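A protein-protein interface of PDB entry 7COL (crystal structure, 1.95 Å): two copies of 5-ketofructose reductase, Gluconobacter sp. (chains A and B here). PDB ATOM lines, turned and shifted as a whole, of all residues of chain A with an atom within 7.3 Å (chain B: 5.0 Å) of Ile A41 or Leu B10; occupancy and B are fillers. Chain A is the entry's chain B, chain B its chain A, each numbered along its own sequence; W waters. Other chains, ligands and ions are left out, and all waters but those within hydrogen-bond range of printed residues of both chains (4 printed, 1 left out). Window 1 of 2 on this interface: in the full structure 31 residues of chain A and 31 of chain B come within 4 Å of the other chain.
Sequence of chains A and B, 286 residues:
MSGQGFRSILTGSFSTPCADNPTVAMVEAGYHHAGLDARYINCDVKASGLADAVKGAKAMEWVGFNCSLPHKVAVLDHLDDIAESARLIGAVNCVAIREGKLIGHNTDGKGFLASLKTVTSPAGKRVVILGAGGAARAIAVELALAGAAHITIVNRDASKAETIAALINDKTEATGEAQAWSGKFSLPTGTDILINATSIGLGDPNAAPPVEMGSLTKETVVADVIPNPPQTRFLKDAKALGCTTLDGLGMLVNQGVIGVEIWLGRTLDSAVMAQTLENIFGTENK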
ATOM      1  N   ILE A   9      -9.197  16.579  -3.210  1.00  0.00           N
ATOM      2  CA  ILE A   9      -7.773  16.322  -3.044  1.00  0.00           C
ATOM      3  C   ILE A   9      -7.164  16.460  -4.448  1.00  0.00           C
ATOM      4  O   ILE A   9      -7.760  16.007  -5.432  1.00  0.00           O
ATOM      5  CB  ILE A   9      -7.520  14.921  -2.402  1.00  0.00           C
ATOM      6  CG1 ILE A   9      -7.955  14.937  -0.928  1.00  0.00           C
ATOM      7  CG2 ILE A   9      -6.052  14.538  -2.483  1.00  0.00           C
ATOM      8  CD1 ILE A   9      -8.589  13.647  -0.445  1.00  0.00           C
ATOM      9  N   LEU A  10      -6.011  17.121  -4.544  1.00  0.00           N
ATOM     10  CA  LEU A  10      -5.394  17.374  -5.840  1.00  0.00           C
ATOM     11  C   LEU A  10      -4.106  16.624  -6.087  1.00  0.00           C
ATOM     12  O   LEU A  10      -3.140  16.692  -5.294  1.00  0.00           O
ATOM     13  CB  LEU A  10      -5.201  18.872  -6.078  1.00  0.00           C
ATOM     14  CG  LEU A  10      -6.483  19.708  -6.069  1.00  0.00           C
ATOM     15  CD1 LEU A  10      -6.124  21.184  -6.160  1.00  0.00           C
ATOM     16  CD2 LEU A  10      -7.444  19.298  -7.196  1.00  0.00           C
ATOM     17  N   THR A  11      -4.114  15.880  -7.184  1.00  0.00           N
ATOM     18  CA  THR A  11      -2.892  15.256  -7.711  1.00  0.00           C
ATOM     19  C   THR A  11      -2.694  15.658  -9.168  1.00  0.00           C
ATOM     20  O   THR A  11      -3.508  16.404  -9.713  1.00  0.00           O
ATOM     21  CB  THR A  11      -2.876  13.723  -7.532  1.00  0.00           C
ATOM     22  OG1 THR A  11      -3.993  13.130  -8.208  1.00  0.00           O
ATOM     23  CG2 THR A  11      -2.916  13.359  -6.036  1.00  0.00           C
ATOM     24  N   GLY A  12      -1.620  15.195  -9.807  1.00  0.00           N
ATOM     25  CA  GLY A  12      -1.405  15.569 -11.193  1.00  0.00           C
ATOM     26  C   GLY A  12      -0.155  15.068 -11.870  1.00  0.00           C
ATOM     27  O   GLY A  12       0.547  14.215 -11.332  1.00  0.00           O
ATOM     28  N   SER A  13       0.089  15.605 -13.066  1.00  0.00           N
ATOM     29  CA  SER A  13       1.267  15.250 -13.858  1.00  0.00           C
ATOM     30  C   SER A  13       1.849  16.468 -14.562  1.00  0.00           C
ATOM     31  O   SER A  13       1.114  17.339 -15.042  1.00  0.00           O
ATOM     32  CB  SER A  13       0.927  14.166 -14.874  1.00  0.00           C
ATOM     33  OG  SER A  13       2.062  13.848 -15.672  1.00  0.00           O
ATOM     34  N   PHE A  14       3.181  16.534 -14.556  1.00  0.00           N
ATOM     35  CA  PHE A  14       3.939  17.489 -15.352  1.00  0.00           C
ATOM     36  C   PHE A  14       4.754  16.693 -16.365  1.00  0.00           C
ATOM     37  O   PHE A  14       5.517  15.810 -15.980  1.00  0.00           O
ATOM     38  CB  PHE A  14       4.888  18.306 -14.475  1.00  0.00           C
ATOM     39  CG  PHE A  14       4.227  19.027 -13.321  1.00  0.00           C
ATOM     40  CD1 PHE A  14       2.948  19.581 -13.444  1.00  0.00           C
ATOM     41  CD2 PHE A  14       4.925  19.200 -12.114  1.00  0.00           C
ATOM     42  CE1 PHE A  14       2.360  20.258 -12.385  1.00  0.00           C
ATOM     43  CE2 PHE A  14       4.346  19.895 -11.055  1.00  0.00           C
ATOM     44  CZ  PHE A  14       3.065  20.415 -11.186  1.00  0.00           C
ATOM     45  N   VAL A  24      -4.175   9.954 -16.335  1.00  0.00           N
ATOM     46  CA  VAL A  24      -5.371  10.649 -15.816  1.00  0.00           C
ATOM     47  C   VAL A  24      -6.627   9.751 -15.821  1.00  0.00           C
ATOM     48  O   VAL A  24      -7.340   9.680 -14.820  1.00  0.00           O
ATOM     49  CB  VAL A  24      -5.662  11.994 -16.528  1.00  0.00           C
ATOM     50  CG1 VAL A  24      -5.860  11.813 -18.040  1.00  0.00           C
ATOM     51  CG2 VAL A  24      -6.888  12.686 -15.914  1.00  0.00           C
ATOM     52  N   GLU A  28      -8.158   8.343 -12.331  1.00  0.00           N
ATOM     53  CA  GLU A  28      -9.479   8.868 -11.971  1.00  0.00           C
ATOM     54  C   GLU A  28     -10.589   7.805 -11.942  1.00  0.00           C
ATOM     55  O   GLU A  28     -11.527   7.924 -11.161  1.00  0.00           O
ATOM     56  CB  GLU A  28      -9.853  10.076 -12.813  1.00  0.00           C
ATOM     57  CG  GLU A  28      -8.959  11.262 -12.492  1.00  0.00           C
ATOM     58  CD  GLU A  28      -9.541  12.594 -12.906  1.00  0.00           C
ATOM     59  OE1 GLU A  28     -10.436  12.627 -13.775  1.00  0.00           O
ATOM     60  OE2 GLU A  28      -9.082  13.610 -12.358  1.00  0.00           O
ATOM     61  N   TYR A  31      -9.921   6.523  -8.449  1.00  0.00           N
ATOM     62  CA  TYR A  31     -10.557   7.463  -7.512  1.00  0.00           C
ATOM     63  C   TYR A  31     -12.069   7.255  -7.386  1.00  0.00           C
ATOM     64  O   TYR A  31     -12.584   7.102  -6.280  1.00  0.00           O
ATOM     65  CB  TYR A  31     -10.247   8.917  -7.891  1.00  0.00           C
ATOM     66  CG  TYR A  31      -8.808   9.393  -7.678  1.00  0.00           C
ATOM     67  CD1 TYR A  31      -7.958   8.775  -6.745  1.00  0.00           C
ATOM     68  CD2 TYR A  31      -8.313  10.497  -8.388  1.00  0.00           C
ATOM     69  CE1 TYR A  31      -6.659   9.231  -6.543  1.00  0.00           C
ATOM     70  CE2 TYR A  31      -7.006  10.964  -8.189  1.00  0.00           C
ATOM     71  CZ  TYR A  31      -6.188  10.324  -7.266  1.00  0.00           C
ATOM     72  OH  TYR A  31      -4.897  10.767  -7.057  1.00  0.00           O
ATOM     73  N   ALA A  38     -10.966  13.139  -5.232  1.00  0.00           N
ATOM     74  CA  ALA A  38      -9.589  13.471  -5.582  1.00  0.00           C
ATOM     75  C   ALA A  38      -9.525  13.594  -7.091  1.00  0.00           C
ATOM     76  O   ALA A  38     -10.283  12.932  -7.802  1.00  0.00           O
ATOM     77  CB  ALA A  38      -8.638  12.383  -5.104  1.00  0.00           C
ATOM     78  N   ARG A  39      -8.628  14.447  -7.578  1.00  0.00           N
ATOM     79  CA  ARG A  39      -8.490  14.654  -9.007  1.00  0.00           C
ATOM     80  C   ARG A  39      -7.043  14.473  -9.447  1.00  0.00           C
ATOM     81  O   ARG A  39      -6.108  14.703  -8.664  1.00  0.00           O
ATOM     82  CB  ARG A  39      -9.028  16.039  -9.399  1.00  0.00           C
ATOM     83  CG  ARG A  39     -10.503  16.223  -9.035  1.00  0.00           C
ATOM     84  CD  ARG A  39     -11.054  17.595  -9.343  1.00  0.00           C
ATOM     85  NE  ARG A  39     -11.370  17.699 -10.762  1.00  0.00           N
ATOM     86  CZ  ARG A  39     -11.926  18.760 -11.338  1.00  0.00           C
ATOM     87  NH1 ARG A  39     -12.239  19.836 -10.621  1.00  0.00           N
ATOM     88  NH2 ARG A  39     -12.163  18.742 -12.642  1.00  0.00           N
ATOM     89  N   TYR A  40      -6.876  14.045 -10.696  1.00  0.00           N
ATOM     90  CA  TYR A  40      -5.546  13.943 -11.314  1.00  0.00           C
ATOM     91  C   TYR A  40      -5.465  14.906 -12.487  1.00  0.00           C
ATOM     92  O   TYR A  40      -6.184  14.755 -13.484  1.00  0.00           O
ATOM     93  CB  TYR A  40      -5.256  12.507 -11.728  1.00  0.00           C
ATOM     94  CG  TYR A  40      -3.855  12.237 -12.204  1.00  0.00           C
ATOM     95  CD1 TYR A  40      -3.491  12.455 -13.545  1.00  0.00           C
ATOM     96  CD2 TYR A  40      -2.882  11.745 -11.328  1.00  0.00           C
ATOM     97  CE1 TYR A  40      -2.198  12.193 -13.991  1.00  0.00           C
ATOM     98  CE2 TYR A  40      -1.588  11.470 -11.768  1.00  0.00           C
ATOM     99  CZ  TYR A  40      -1.253  11.695 -13.094  1.00  0.00           C
ATOM    100  OH  TYR A  40       0.022  11.405 -13.536  1.00  0.00           O
ATOM    101  N   ILE A  41      -4.586  15.894 -12.361  1.00  0.00           N
ATOM    102  CA  ILE A  41      -4.521  17.005 -13.317  1.00  0.00           C
ATOM    103  C   ILE A  41      -3.342  16.851 -14.276  1.00  0.00           C
ATOM    104  O   ILE A  41      -2.193  17.108 -13.904  1.00  0.00           O
ATOM    105  CB  ILE A  41      -4.451  18.389 -12.596  1.00  0.00           C
ATOM    106  CG1 ILE A  41      -5.451  18.494 -11.418  1.00  0.00           C
ATOM    107  CG2 ILE A  41      -4.604  19.553 -13.577  1.00  0.00           C
ATOM    108  CD1 ILE A  41      -6.892  18.124 -11.731  1.00  0.00           C
ATOM    109  N   ASN A  42      -3.650  16.441 -15.505  1.00  0.00           N
ATOM    110  CA  ASN A  42      -2.656  16.267 -16.566  1.00  0.00           C
ATOM    111  C   ASN A  42      -2.192  17.584 -17.227  1.00  0.00           C
ATOM    112  O   ASN A  42      -2.880  18.129 -18.103  1.00  0.00           O
ATOM    113  CB  ASN A  42      -3.199  15.286 -17.618  1.00  0.00           C
ATOM    114  CG  ASN A  42      -2.112  14.745 -18.542  1.00  0.00           C
ATOM    115  OD1 ASN A  42      -0.930  14.705 -18.189  1.00  0.00           O
ATOM    116  ND2 ASN A  42      -2.516  14.331 -19.731  1.00  0.00           N
ATOM    117  N   CYS A  43      -1.014  18.074 -16.824  1.00  0.00           N
ATOM    118  CA  CYS A  43      -0.488  19.361 -17.317  1.00  0.00           C
ATOM    119  C   CYS A  43       0.626  19.241 -18.344  1.00  0.00           C
ATOM    120  O   CYS A  43       1.579  18.479 -18.149  1.00  0.00           O
ATOM    121  CB  CYS A  43       0.049  20.209 -16.164  1.00  0.00           C
ATOM    122  SG  CYS A  43      -1.141  20.415 -14.832  1.00  0.00           S
ATOM    123  N   ASP A  44       0.513  20.030 -19.417  1.00  0.00           N
ATOM    124  CA  ASP A  44       1.599  20.170 -20.370  1.00  0.00           C
ATOM    125  C   ASP A  44       2.563  21.231 -19.842  1.00  0.00           C
ATOM    126  O   ASP A  44       2.243  22.432 -19.804  1.00  0.00           O
ATOM    127  CB  ASP A  44       1.075  20.489 -21.775  1.00  0.00           C
ATOM    128  CG  ASP A  44       1.996  19.961 -22.861  1.00  0.00           C
ATOM    129  OD1 ASP A  44       3.102  20.511 -23.041  1.00  0.00           O
ATOM    130  OD2 ASP A  44       1.624  18.983 -23.511  1.00  0.00           O
ATOM    131  N   TRP A  62      -1.543  20.653  -3.687  1.00  0.00           N
ATOM    132  CA  TRP A  62      -1.532  19.287  -4.213  1.00  0.00           C
ATOM    133  C   TRP A  62      -0.806  18.405  -3.218  1.00  0.00           C
ATOM    134  O   TRP A  62       0.030  18.891  -2.459  1.00  0.00           O
ATOM    135  CB  TRP A  62      -0.799  19.225  -5.547  1.00  0.00           C
ATOM    136  CG  TRP A  62      -1.419  19.954  -6.703  1.00  0.00           C
ATOM    137  CD1 TRP A  62      -2.256  21.057  -6.659  1.00  0.00           C
ATOM    138  CD2 TRP A  62      -1.185  19.688  -8.084  1.00  0.00           C
ATOM    139  NE1 TRP A  62      -2.579  21.450  -7.934  1.00  0.00           N
ATOM    140  CE2 TRP A  62      -1.913  20.642  -8.825  1.00  0.00           C
ATOM    141  CE3 TRP A  62      -0.422  18.724  -8.777  1.00  0.00           C
ATOM    142  CZ2 TRP A  62      -1.925  20.651 -10.226  1.00  0.00           C
ATOM    143  CZ3 TRP A  62      -0.413  18.751 -10.168  1.00  0.00           C
ATOM    144  CH2 TRP A  62      -1.165  19.703 -10.879  1.00  0.00           C
ATOM    145  N   GLY A  64       0.654  15.485  -4.403  1.00  0.00           N
ATOM    146  CA  GLY A  64       1.691  14.844  -5.209  1.00  0.00           C
ATOM    147  C   GLY A  64       1.463  15.009  -6.685  1.00  0.00           C
ATOM    148  O   GLY A  64       0.403  15.473  -7.116  1.00  0.00           O
ATOM    149  N   PHE A  65       2.472  14.621  -7.465  1.00  0.00           N
ATOM    150  CA  PHE A  65       2.400  14.687  -8.918  1.00  0.00           C
ATOM    151  C   PHE A  65       3.399  13.714  -9.535  1.00  0.00           C
ATOM    152  O   PHE A  65       4.406  13.379  -8.916  1.00  0.00           O
ATOM    153  CB  PHE A  65       2.619  16.128  -9.428  1.00  0.00           C
ATOM    154  CG  PHE A  65       3.936  16.758  -8.997  1.00  0.00           C
ATOM    155  CD1 PHE A  65       4.034  17.474  -7.796  1.00  0.00           C
ATOM    156  CD2 PHE A  65       5.084  16.643  -9.800  1.00  0.00           C
ATOM    157  CE1 PHE A  65       5.243  18.051  -7.401  1.00  0.00           C
ATOM    158  CE2 PHE A  65       6.296  17.222  -9.409  1.00  0.00           C
ATOM    159  CZ  PHE A  65       6.368  17.934  -8.212  1.00  0.00           C
ATOM    160  N   ASN A  66       3.082  13.250 -10.739  1.00  0.00           N
ATOM    161  CA  ASN A  66       4.019  12.509 -11.575  1.00  0.00           C
ATOM    162  C   ASN A  66       4.844  13.467 -12.434  1.00  0.00           C
ATOM    163  O   ASN A  66       4.453  14.626 -12.677  1.00  0.00           O
ATOM    164  CB  ASN A  66       3.282  11.532 -12.507  1.00  0.00           C
ATOM    165  CG  ASN A  66       2.750  10.300 -11.800  1.00  0.00           C
ATOM    166  OD1 ASN A  66       1.573   9.983 -11.935  1.00  0.00           O
ATOM    167  ND2 ASN A  66       3.621   9.562 -11.093  1.00  0.00           N
ATOM    168  N   SER B   8      -6.850  18.067 -21.118  1.00  0.00           N
ATOM    169  CA  SER B   8      -8.036  18.920 -20.958  1.00  0.00           C
ATOM    170  C   SER B   8      -7.616  20.370 -20.813  1.00  0.00           C
ATOM    171  O   SER B   8      -6.519  20.658 -20.324  1.00  0.00           O
ATOM    172  CB  SER B   8      -8.844  18.532 -19.708  1.00  0.00           C
ATOM    173  OG  SER B   8      -9.118  17.137 -19.597  1.00  0.00           O
ATOM    174  N   ILE B   9      -8.494  21.285 -21.221  1.00  0.00           N
ATOM    175  CA  ILE B   9      -8.339  22.714 -20.921  1.00  0.00           C
ATOM    176  C   ILE B   9      -8.457  22.902 -19.407  1.00  0.00           C
ATOM    177  O   ILE B   9      -9.396  22.392 -18.783  1.00  0.00           O
ATOM    178  CB  ILE B   9      -9.416  23.572 -21.622  1.00  0.00           C
ATOM    179  CG1 ILE B   9      -9.286  23.488 -23.147  1.00  0.00           C
ATOM    180  CG2 ILE B   9      -9.304  25.032 -21.200  1.00  0.00           C
ATOM    181  CD1 ILE B   9     -10.616  23.401 -23.858  1.00  0.00           C
ATOM    182  N   LEU B  10      -7.501  23.628 -18.826  1.00  0.00           N
ATOM    183  CA  LEU B  10      -7.438  23.803 -17.391  1.00  0.00           C
ATOM    184  C   LEU B  10      -7.827  25.218 -16.981  1.00  0.00           C
ATOM    185  O   LEU B  10      -7.350  26.205 -17.538  1.00  0.00           O
ATOM    186  CB  LEU B  10      -6.061  23.443 -16.885  1.00  0.00           C
ATOM    187  CG  LEU B  10      -5.653  21.987 -17.156  1.00  0.00           C
ATOM    188  CD1 LEU B  10      -4.299  21.796 -16.508  1.00  0.00           C
ATOM    189  CD2 LEU B  10      -6.667  20.992 -16.603  1.00  0.00           C
ATOM    190  N   THR B  11      -8.772  25.286 -16.066  1.00  0.00           N
ATOM    191  CA  THR B  11      -9.210  26.542 -15.474  1.00  0.00           C
ATOM    192  C   THR B  11      -9.276  26.247 -13.977  1.00  0.00           C
ATOM    193  O   THR B  11      -9.030  25.103 -13.557  1.00  0.00           O
ATOM    194  CB  THR B  11     -10.585  27.001 -16.000  1.00  0.00           C
ATOM    195  OG1 THR B  11     -11.581  26.010 -15.729  1.00  0.00           O
ATOM    196  CG2 THR B  11     -10.535  27.302 -17.491  1.00  0.00           C
ATOM    197  N   GLY B  12      -9.598  27.253 -13.176  1.00  0.00           N
ATOM    198  CA  GLY B  12      -9.789  27.012 -11.758  1.00  0.00           C
ATOM    199  C   GLY B  12     -10.048  28.204 -10.896  1.00  0.00           C
ATOM    200  O   GLY B  12     -10.493  29.247 -11.380  1.00  0.00           O
ATOM    201  N   ARG B  39     -11.712  21.610 -17.559  1.00  0.00           N
ATOM    202  CA  ARG B  39     -11.872  21.340 -16.130  1.00  0.00           C
ATOM    203  C   ARG B  39     -11.695  22.618 -15.330  1.00  0.00           C
ATOM    204  O   ARG B  39     -10.953  23.536 -15.738  1.00  0.00           O
ATOM    205  CB  ARG B  39     -10.846  20.311 -15.632  1.00  0.00           C
ATOM    206  CG  ARG B  39     -10.747  19.044 -16.459  1.00  0.00           C
ATOM    207  CD  ARG B  39      -9.698  18.101 -15.903  1.00  0.00           C
ATOM    208  NE  ARG B  39     -10.124  17.524 -14.629  1.00  0.00           N
ATOM    209  CZ  ARG B  39      -9.634  16.400 -14.115  1.00  0.00           C
ATOM    210  NH1 ARG B  39     -10.106  15.951 -12.957  1.00  0.00           N
ATOM    211  NH2 ARG B  39      -8.670  15.737 -14.743  1.00  0.00           N
ATOM    212  N   ILE B  41     -10.582  23.748 -11.519  1.00  0.00           N
ATOM    213  CA  ILE B  41      -9.831  23.228 -10.374  1.00  0.00           C
ATOM    214  C   ILE B  41      -9.949  24.190  -9.202  1.00  0.00           C
ATOM    215  O   ILE B  41      -9.362  25.274  -9.206  1.00  0.00           O
ATOM    216  CB  ILE B  41      -8.331  22.950 -10.737  1.00  0.00           C
ATOM    217  CG1 ILE B  41      -8.211  22.054 -11.984  1.00  0.00           C
ATOM    218  CG2 ILE B  41      -7.560  22.334  -9.568  1.00  0.00           C
ATOM    219  CD1 ILE B  41      -9.022  20.766 -11.924  1.00  0.00           C
ATOM    220  N   MET B  60       1.601  25.694 -15.792  1.00  0.00           N
ATOM    221  CA  MET B  60       0.771  24.524 -16.035  1.00  0.00           C
ATOM    222  C   MET B  60      -0.120  24.742 -17.244  1.00  0.00           C
ATOM    223  O   MET B  60      -0.956  23.882 -17.582  1.00  0.00           O
ATOM    224  CB  MET B  60      -0.093  24.201 -14.810  1.00  0.00           C
ATOM    225  CG  MET B  60       0.638  23.597 -13.612  1.00  0.00           C
ATOM    226  SD  MET B  60      -0.515  23.577 -12.233  1.00  0.00           S
ATOM    227  CE  MET B  60       0.579  23.523 -10.811  1.00  0.00           C
ATOM    228  N   TRP B  62      -2.673  26.723 -17.835  1.00  0.00           N
ATOM    229  CA  TRP B  62      -4.082  27.065 -17.626  1.00  0.00           C
ATOM    230  C   TRP B  62      -4.451  28.249 -18.529  1.00  0.00           C
ATOM    231  O   TRP B  62      -3.591  29.067 -18.859  1.00  0.00           O
ATOM    232  CB  TRP B  62      -4.333  27.483 -16.173  1.00  0.00           C
ATOM    233  CG  TRP B  62      -4.206  26.407 -15.097  1.00  0.00           C
ATOM    234  CD1 TRP B  62      -3.414  25.283 -15.125  1.00  0.00           C
ATOM    235  CD2 TRP B  62      -4.857  26.396 -13.817  1.00  0.00           C
ATOM    236  NE1 TRP B  62      -3.556  24.570 -13.966  1.00  0.00           N
ATOM    237  CE2 TRP B  62      -4.429  25.231 -13.140  1.00  0.00           C
ATOM    238  CE3 TRP B  62      -5.785  27.248 -13.184  1.00  0.00           C
ATOM    239  CZ2 TRP B  62      -4.885  24.896 -11.849  1.00  0.00           C
ATOM    240  CZ3 TRP B  62      -6.233  26.924 -11.902  1.00  0.00           C
ATOM    241  CH2 TRP B  62      -5.789  25.752 -11.249  1.00  0.00           C
ATOM    242  N   VAL B  63      -5.723  28.340 -18.912  1.00  0.00           N
ATOM    243  CA  VAL B  63      -6.185  29.459 -19.757  1.00  0.00           C
ATOM    244  C   VAL B  63      -6.823  30.574 -18.938  1.00  0.00           C
ATOM    245  O   VAL B  63      -7.081  31.671 -19.454  1.00  0.00           O
ATOM    246  CB  VAL B  63      -7.115  28.995 -20.910  1.00  0.00           C
ATOM    247  CG1 VAL B  63      -6.391  27.996 -21.812  1.00  0.00           C
ATOM    248  CG2 VAL B  63      -8.413  28.419 -20.372  1.00  0.00           C
ATOM    249  N   GLY B  64      -7.056  30.298 -17.661  1.00  0.00           N
ATOM    250  CA  GLY B  64      -7.657  31.285 -16.757  1.00  0.00           C
ATOM    251  C   GLY B  64      -8.028  30.728 -15.401  1.00  0.00           C
ATOM    252  O   GLY B  64      -8.004  29.522 -15.184  1.00  0.00           O
HETATM  253  O   HOH W   1     -10.421  14.200 -16.236  1.00  0.00           O
HETATM  254  O   HOH W   2      -1.481  21.999 -19.528  1.00  0.00           O
HETATM  255  O   HOH W   3      -6.470  16.636 -16.610  1.00  0.00           O
HETATM  256  O   HOH W   4      -5.532  18.492 -18.674  1.00  0.00           O
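The side-chain carboxylate (OE2) of Glu A28 lies within salt-bridge range of the guanidinium group (NH1) of Arg B39, 2.6 Å away. The guanidinium group of Arg B39 is in hydrogen-bond range of the backbone carbonyl oxygen of Tyr A40 (3.0 Å). The guanidinium group (NH1) of Arg B39 lies close to the guanidinium group (NE) of Arg A39 (3.1 Å).
The backbone carbonyl oxygen (O) of Arg B39 lies within hydrogen-bond range of the side-chain hydroxyl (OG1) of Thr B11, at 2.6 Å. O of Thr B11 is in hydrogen-bond range of N of Ile B41, at 2.9 Å. The backbone carbonyl oxygen (O) of Ile A9 is in hydrogen-bond range of the backbone NH (N) of Arg A39 (2.8 Å). The side-chain hydroxyl (OG1) of Thr A11 is in hydrogen-bond range of the backbone carbonyl oxygen (O) of Arg A39, at 2.7 Å. N of Phe A14 lies within hydrogen-bond range of O of Asn A66. O of Ile A41 sits at hydrogen-bond distance from SG of Cys A43 (3.6 Å).
CG2 of Ile B41 touches CD2 of Leu A10 (3.9 Å). CG of Met B60 touches CE1 of Phe A14, at 3.95 Å. Val A24 touches Arg B39. CD1 of Ile B41 touches CZ of Arg A39, at 3.6 Å. Ile A41 touches Leu B10 (CG2 to CD1, 3.7 Å). CD1 of Ile A41 touches CD1 of Ile B41, 3.4 Å away. SG of Cys A43 touches CD1 of Leu B10, 3.8 Å away. Cys A43 touches Met B60. Trp A62 touches Met B60.
Ile A41 touches two residues of chain B. Of chain A, only Ile A41 (3.7 Å) and Cys A43 (3.8 Å) come within 4 Å of Leu B10. Printed residues of chain A within 4 Å of Arg B39: Val A24 (3.7 Å), Glu A28 (2.6 Å), Arg A39 (3.1 Å) and Tyr A40 (3.0 Å). Of the printed residues of chain B, Trp A62 touches Met B60. Of the printed residues of chain B, Arg A39 touches Arg B39 and Ile B41. Printed residues of chain B within 4 Å of Glu A28: Arg B39. The nearest residue of chain B that does not touch Ile A41 is Arg B39 (4.02 Å). The nearest printed residue of chain B that does not touch Arg A39 is Thr B11 (6.8 Å).
Hydrophobic or aromatic side chains of chain B within 4 Å of the printed part of chain A: Leu B10, Ile B41 and Met B60. Of the 20 printed residues of chain A, 9 touch a printed residue of chain B. Along chain A the printed residues that touch a printed residue of chain B span positions 10 to 62.
Leu A10 touches Ile B41, and with the chains exchanged Ile A41 touches Leu B10. Arg A39 touches its own counterpart, Arg B39. Arg A39 touches Ile B41, but with the chains exchanged Ile A41 does not touch Arg B39 (4.02 Å). Ile B41 touches its own counterpart, Ile A41. Of the 12 pairs that touch across the chains among the printed residues, 4 have their exchanged pair printed and touching as well.
Water W4 bridges the backbone carbonyl oxygen (O) of Asn A42 (2.7 Å) and the backbone NH (N) of Ser B8 (2.8 Å). Water W2 bridges the backbone carbonyl oxygen (O) of Met B60 (2.8 Å) and the backbone NH (N) of Asp A44 (2.8 Å). Water W1 lies within hydrogen-bond range of NH2 of Arg B39 and OE1 of Glu A28. Water W3 lies within hydrogen-bond range of the guanidinium group of Arg B39 (3.0 Å) and the backbone NH of Asn A42 (3.0 Å).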
